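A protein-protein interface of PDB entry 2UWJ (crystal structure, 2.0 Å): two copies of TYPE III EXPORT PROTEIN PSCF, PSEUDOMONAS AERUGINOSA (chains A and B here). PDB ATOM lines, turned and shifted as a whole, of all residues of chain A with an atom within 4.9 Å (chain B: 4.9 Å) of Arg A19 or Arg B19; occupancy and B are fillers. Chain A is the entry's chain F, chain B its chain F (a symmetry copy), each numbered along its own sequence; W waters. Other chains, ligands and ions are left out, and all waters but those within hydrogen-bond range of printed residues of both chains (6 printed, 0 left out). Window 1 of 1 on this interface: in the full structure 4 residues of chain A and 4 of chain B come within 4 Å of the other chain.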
ATOM      1  N   SER A  15     -16.311 -31.366 -18.183  1.00  0.00           N
ATOM      2  CA  SER A  15     -17.053 -30.679 -19.241  1.00  0.00           C
ATOM      3  C   SER A  15     -18.015 -29.617 -18.753  1.00  0.00           C
ATOM      4  O   SER A  15     -18.293 -28.665 -19.469  1.00  0.00           O
ATOM      5  CB  SER A  15     -17.795 -31.703 -20.132  1.00  0.00           C
ATOM      6  OG  SER A  15     -18.616 -32.547 -19.328  1.00  0.00           O
ATOM      7  N   THR A  16     -18.536 -29.774 -17.553  1.00  0.00           N
ATOM      8  CA  THR A  16     -19.469 -28.781 -17.022  1.00  0.00           C
ATOM      9  C   THR A  16     -18.729 -27.473 -16.766  1.00  0.00           C
ATOM     10  O   THR A  16     -19.189 -26.383 -17.115  1.00  0.00           O
ATOM     11  CB  THR A  16     -20.107 -29.294 -15.680  1.00  0.00           C
ATOM     12  OG1 THR A  16     -20.941 -30.422 -15.981  1.00  0.00           O
ATOM     13  CG2 THR A  16     -20.957 -28.225 -15.071  1.00  0.00           C
ATOM     14  N   VAL A  17     -17.554 -27.592 -16.177  1.00  0.00           N
ATOM     15  CA  VAL A  17     -16.735 -26.425 -15.871  1.00  0.00           C
ATOM     16  C   VAL A  17     -16.170 -25.817 -17.162  1.00  0.00           C
ATOM     17  O   VAL A  17     -16.201 -24.596 -17.331  1.00  0.00           O
ATOM     18  CB  VAL A  17     -15.580 -26.805 -14.858  1.00  0.00           C
ATOM     19  CG1 VAL A  17     -14.645 -25.618 -14.610  1.00  0.00           C
ATOM     20  CG2 VAL A  17     -16.211 -27.270 -13.556  1.00  0.00           C
ATOM     21  N   THR A  18     -15.673 -26.639 -18.073  1.00  0.00           N
ATOM     22  CA  THR A  18     -15.140 -26.065 -19.307  1.00  0.00           C
ATOM     23  C   THR A  18     -16.243 -25.434 -20.147  1.00  0.00           C
ATOM     24  O   THR A  18     -15.990 -24.459 -20.844  1.00  0.00           O
ATOM     25  CB  THR A  18     -14.412 -27.098 -20.153  1.00  0.00           C
ATOM     26  OG1 THR A  18     -15.326 -28.102 -20.556  1.00  0.00           O
ATOM     27  CG2 THR A  18     -13.316 -27.764 -19.295  1.00  0.00           C
ATOM     28  N   ARG A  19     -17.459 -25.984 -20.078  1.00  0.00           N
ATOM     29  CA  ARG A  19     -18.567 -25.389 -20.818  1.00  0.00           C
ATOM     30  C   ARG A  19     -18.860 -24.002 -20.272  1.00  0.00           C
ATOM     31  O   ARG A  19     -19.114 -23.088 -21.061  1.00  0.00           O
ATOM     32  CB  ARG A  19     -19.856 -26.251 -20.771  1.00  0.00           C
ATOM     33  CG  ARG A  19     -21.002 -25.675 -21.750  1.00  0.00           C
ATOM     34  CD  ARG A  19     -22.192 -26.684 -21.892  1.00  0.00           C
ATOM     35  NE  ARG A  19     -21.720 -27.966 -22.404  1.00  0.00           N
ATOM     36  CZ  ARG A  19     -21.585 -29.083 -21.667  1.00  0.00           C
ATOM     37  NH1 ARG A  19     -21.921 -29.147 -20.374  1.00  0.00           N
ATOM     38  NH2 ARG A  19     -20.975 -30.133 -22.192  1.00  0.00           N
ATOM     39  N   ALA A  20     -18.845 -23.821 -18.931  1.00  0.00           N
ATOM     40  CA  ALA A  20     -19.078 -22.484 -18.345  1.00  0.00           C
ATOM     41  C   ALA A  20     -17.946 -21.531 -18.805  1.00  0.00           C
ATOM     42  O   ALA A  20     -18.187 -20.359 -19.182  1.00  0.00           O
ATOM     43  CB  ALA A  20     -19.100 -22.559 -16.813  1.00  0.00           C
ATOM     44  N   LEU A  21     -16.712 -22.035 -18.804  1.00  0.00           N
ATOM     45  CA  LEU A  21     -15.593 -21.226 -19.285  1.00  0.00           C
ATOM     46  C   LEU A  21     -15.812 -20.840 -20.780  1.00  0.00           C
ATOM     47  O   LEU A  21     -15.573 -19.693 -21.189  1.00  0.00           O
ATOM     48  CB  LEU A  21     -14.253 -21.998 -19.130  1.00  0.00           C
ATOM     49  CG  LEU A  21     -12.982 -21.165 -19.480  1.00  0.00           C
ATOM     50  CD1 LEU A  21     -12.810 -20.007 -18.413  1.00  0.00           C
ATOM     51  CD2 LEU A  21     -11.696 -22.076 -19.461  1.00  0.00           C
ATOM     52  N   ARG A  22     -16.259 -21.785 -21.599  1.00  0.00           N
ATOM     53  CA  ARG A  22     -16.487 -21.469 -23.018  1.00  0.00           C
ATOM     54  C   ARG A  22     -17.589 -20.425 -23.172  1.00  0.00           C
ATOM     55  O   ARG A  22     -17.526 -19.538 -24.034  1.00  0.00           O
ATOM     56  CB  ARG A  22     -16.857 -22.748 -23.774  1.00  0.00           C
ATOM     57  CG  ARG A  22     -15.615 -23.684 -23.955  1.00  0.00           C
ATOM     58  CD  ARG A  22     -16.020 -25.076 -24.449  1.00  0.00           C
ATOM     59  NE  ARG A  22     -16.959 -24.943 -25.536  1.00  0.00           N
ATOM     60  CZ  ARG A  22     -18.116 -25.592 -25.637  1.00  0.00           C
ATOM     61  NH1 ARG A  22     -18.520 -26.478 -24.696  1.00  0.00           N
ATOM     62  NH2 ARG A  22     -18.881 -25.331 -26.692  1.00  0.00           N
ATOM     63  N   ASP A  23     -18.607 -20.524 -22.330  1.00  0.00           N
ATOM     64  CA  ASP A  23     -19.718 -19.568 -22.372  1.00  0.00           C
ATOM     65  C   ASP A  23     -19.162 -18.127 -22.144  1.00  0.00           C
ATOM     66  O   ASP A  23     -19.532 -17.170 -22.870  1.00  0.00           O
ATOM     67  CB  ASP A  23     -20.700 -19.960 -21.266  1.00  0.00           C
ATOM     68  CG  ASP A  23     -22.056 -19.351 -21.442  1.00  0.00           C
ATOM     69  OD1 ASP A  23     -22.235 -18.533 -22.374  1.00  0.00           O
ATOM     70  OD2 ASP A  23     -22.943 -19.677 -20.626  1.00  0.00           O
ATOM     71  N   SER B  15     -29.320 -23.359 -14.801  1.00  0.00           N
ATOM     72  CA  SER B  15     -28.353 -22.828 -15.763  1.00  0.00           C
ATOM     73  C   SER B  15     -27.384 -23.849 -16.316  1.00  0.00           C
ATOM     74  O   SER B  15     -26.902 -23.697 -17.431  1.00  0.00           O
ATOM     75  CB  SER B  15     -27.581 -21.637 -15.148  1.00  0.00           C
ATOM     76  OG  SER B  15     -26.986 -22.024 -13.911  1.00  0.00           O
ATOM     77  N   THR B  16     -27.081 -24.879 -15.551  1.00  0.00           N
ATOM     78  CA  THR B  16     -26.154 -25.903 -16.029  1.00  0.00           C
ATOM     79  C   THR B  16     -26.795 -26.671 -17.181  1.00  0.00           C
ATOM     80  O   THR B  16     -26.180 -26.923 -18.219  1.00  0.00           O
ATOM     81  CB  THR B  16     -25.795 -26.900 -14.868  1.00  0.00           C
ATOM     82  OG1 THR B  16     -25.037 -26.186 -13.882  1.00  0.00           O
ATOM     83  CG2 THR B  16     -24.954 -28.020 -15.393  1.00  0.00           C
ATOM     84  N   VAL B  17     -28.055 -27.017 -16.999  1.00  0.00           N
ATOM     85  CA  VAL B  17     -28.796 -27.755 -18.015  1.00  0.00           C
ATOM     86  C   VAL B  17     -29.082 -26.855 -19.225  1.00  0.00           C
ATOM     87  O   VAL B  17     -28.905 -27.284 -20.368  1.00  0.00           O
ATOM     88  CB  VAL B  17     -30.130 -28.351 -17.411  1.00  0.00           C
ATOM     89  CG1 VAL B  17     -30.973 -29.036 -18.489  1.00  0.00           C
ATOM     90  CG2 VAL B  17     -29.766 -29.335 -16.311  1.00  0.00           C
ATOM     91  N   THR B  18     -29.504 -25.620 -18.998  1.00  0.00           N
ATOM     92  CA  THR B  18     -29.770 -24.757 -20.146  1.00  0.00           C
ATOM     93  C   THR B  18     -28.490 -24.426 -20.901  1.00  0.00           C
ATOM     94  O   THR B  18     -28.531 -24.249 -22.113  1.00  0.00           O
ATOM     95  CB  THR B  18     -30.449 -23.458 -19.742  1.00  0.00           C
ATOM     96  OG1 THR B  18     -29.585 -22.721 -18.897  1.00  0.00           O
ATOM     97  CG2 THR B  18     -31.730 -23.789 -18.947  1.00  0.00           C
ATOM     98  N   ARG B  19     -27.360 -24.346 -20.192  1.00  0.00           N
ATOM     99  CA  ARG B  19     -26.095 -24.084 -20.870  1.00  0.00           C
ATOM    100  C   ARG B  19     -25.761 -25.246 -21.791  1.00  0.00           C
ATOM    101  O   ARG B  19     -25.295 -25.010 -22.908  1.00  0.00           O
ATOM    102  CB  ARG B  19     -24.921 -23.846 -19.884  1.00  0.00           C
ATOM    103  CG  ARG B  19     -23.581 -23.371 -20.647  1.00  0.00           C
ATOM    104  CD  ARG B  19     -22.488 -22.887 -19.635  1.00  0.00           C
ATOM    105  NE  ARG B  19     -22.994 -21.788 -18.820  1.00  0.00           N
ATOM    106  CZ  ARG B  19     -23.354 -21.895 -17.528  1.00  0.00           C
ATOM    107  NH1 ARG B  19     -23.240 -23.031 -16.831  1.00  0.00           N
ATOM    108  NH2 ARG B  19     -23.971 -20.881 -16.944  1.00  0.00           N
ATOM    109  N   ALA B  20     -25.975 -26.505 -21.344  1.00  0.00           N
ATOM    110  CA  ALA B  20     -25.710 -27.672 -22.213  1.00  0.00           C
ATOM    111  C   ALA B  20     -26.654 -27.607 -23.440  1.00  0.00           C
ATOM    112  O   ALA B  20     -26.242 -27.853 -24.598  1.00  0.00           O
ATOM    113  CB  ALA B  20     -25.943 -28.981 -21.449  1.00  0.00           C
ATOM    114  N   LEU B  21     -27.915 -27.250 -23.196  1.00  0.00           N
ATOM    115  CA  LEU B  21     -28.857 -27.101 -24.305  1.00  0.00           C
ATOM    116  C   LEU B  21     -28.363 -25.994 -25.285  1.00  0.00           C
ATOM    117  O   LEU B  21     -28.419 -26.151 -26.515  1.00  0.00           O
ATOM    118  CB  LEU B  21     -30.273 -26.742 -23.775  1.00  0.00           C
ATOM    119  CG  LEU B  21     -31.384 -26.703 -24.869  1.00  0.00           C
ATOM    120  CD1 LEU B  21     -31.612 -28.168 -25.429  1.00  0.00           C
ATOM    121  CD2 LEU B  21     -32.738 -26.166 -24.271  1.00  0.00           C
ATOM    122  N   ARG B  22     -27.883 -24.873 -24.756  1.00  0.00           N
ATOM    123  CA  ARG B  22     -27.400 -23.801 -25.640  1.00  0.00           C
ATOM    124  C   ARG B  22     -26.190 -24.265 -26.446  1.00  0.00           C
ATOM    125  O   ARG B  22     -26.026 -23.922 -27.625  1.00  0.00           O
ATOM    126  CB  ARG B  22     -27.038 -22.571 -24.801  1.00  0.00           C
ATOM    127  CG  ARG B  22     -28.321 -21.850 -24.263  1.00  0.00           C
ATOM    128  CD  ARG B  22     -27.978 -20.801 -23.202  1.00  0.00           C
ATOM    129  NE  ARG B  22     -26.867 -20.002 -23.659  1.00  0.00           N
ATOM    130  CZ  ARG B  22     -25.778 -19.721 -22.948  1.00  0.00           C
ATOM    131  NH1 ARG B  22     -25.621 -20.168 -21.680  1.00  0.00           N
ATOM    132  NH2 ARG B  22     -24.831 -18.994 -23.532  1.00  0.00           N
ATOM    133  N   ASP B  23     -25.337 -25.056 -25.813  1.00  0.00           N
ATOM    134  CA  ASP B  23     -24.145 -25.578 -26.490  1.00  0.00           C
ATOM    135  C   ASP B  23     -24.588 -26.403 -27.740  1.00  0.00           C
ATOM    136  O   ASP B  23     -24.014 -26.253 -28.848  1.00  0.00           O
ATOM    137  CB  ASP B  23     -23.398 -26.459 -25.486  1.00  0.00           C
ATOM    138  CG  ASP B  23     -21.979 -26.724 -25.881  1.00  0.00           C
ATOM    139  OD1 ASP B  23     -21.573 -26.309 -26.991  1.00  0.00           O
ATOM    140  OD2 ASP B  23     -21.272 -27.372 -25.082  1.00  0.00           O
HETATM  141  O   HOH W   1     -21.372 -23.163 -27.514  1.00  0.00           O
HETATM  142  O   HOH W   2     -19.763 -29.914 -24.989  1.00  0.00           O
HETATM  143  O   HOH W   3     -24.687 -18.413 -18.599  1.00  0.00           O
HETATM  144  O   HOH W   4     -22.041 -19.538 -25.402  1.00  0.00           O
HETATM  145  O   HOH W   5     -23.469 -27.400 -18.562  1.00  0.00           O
HETATM  146  O   HOH W   6     -21.842 -25.594 -17.291  1.00  0.00           O
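The guanidinium group (NE) of Arg B19 is in salt-bridge range of the side-chain carboxylate (OD2) of Asp A23.
The side-chain carboxylate (OD1) of Asp A23 lies within salt-bridge range of the guanidinium group (NH2) of Arg B22, at 2.9 Å.
NH2 of Arg A22 is in salt-bridge range of OD1 of Asp B23 (2.9 Å).
NE of Arg A19 is in salt-bridge range of OD2 of Asp B23 (2.8 Å).
Among the printed residues, merely in contact across the chains: Arg A19 with Arg B19, Arg A19 with Ala B20 and Ala A20 with Arg B19.
Of chain B, only Arg B19 (3.6 Å), Ala B20 (3.7 Å) and Asp B23 (2.8 Å) come within 4 Å of Arg A19.
Of the printed residues of chain B, Arg A22 touches Asp B23 (2.9 Å).
Ser B15 touches none of the printed residues of chain A.
Arg B19 touches just these residues of chain A: Arg A19 (3.6 Å), Ala A20 (3.7 Å) and Asp A23 (2.8 Å).
Leu B21 touches none of the printed residues of chain A.
Of the printed residues of chain A, Arg B22 touches Asp A23.
Printed residues of chain A within 4 Å of Asp B23: Arg A19 (2.8 Å) and Arg A22 (2.9 Å).
The nearest printed residue of chain A that does not touch Arg B19 is Thr A16 (5.3 Å).
Of the 9 printed residues of chain B, 4 touch a printed residue of chain A.
Along chain A the printed residues that touch a printed residue of chain B span positions 19 to 23.
Among the printed residues, Asp or Glu carboxylates within 4 Å of a Lys or Arg side-chain nitrogen of the other chain: Arg A19 with Asp B23, Arg A22 with Asp B23, Asp A23 with Arg B19 and Asp A23 with Arg B22.
Arg A19 touches its own counterpart, Arg B19.
Arg A19 touches Ala B20, and with the chains exchanged Ala A20 touches Arg B19.
Arg A19 touches Asp B23, and with the chains exchanged Asp A23 touches Arg B19.
Arg A22 touches Asp B23, and with the chains exchanged Asp A23 touches Arg B22.
9 positions are printed for both chains.
Water W6 bridges the backbone carbonyl oxygen of Thr A16 and the guanidinium group of Arg B19.
Water W5 lies within hydrogen-bond range of O of Thr B16 and NH1 of Arg A19.
Water W2 bridges OD2 of Asp B23 (3.0 Å) and NH2 of Arg A19 (3.1 Å).
Water W3 bridges the side-chain carboxylate of Asp A23 (3.0 Å) and the guanidinium group of Arg B19 (3.1 Å).
Water W1 lies within hydrogen-bond range of the side-chain carboxylate (OD1) of Asp B23 (3.2 Å) and the guanidinium group (NH2) of Arg A22 (3.4 Å).
Water W4 lies within hydrogen-bond range of the side-chain carboxylate (OD1) of Asp A23 and the guanidinium group (NH2) of Arg B22.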
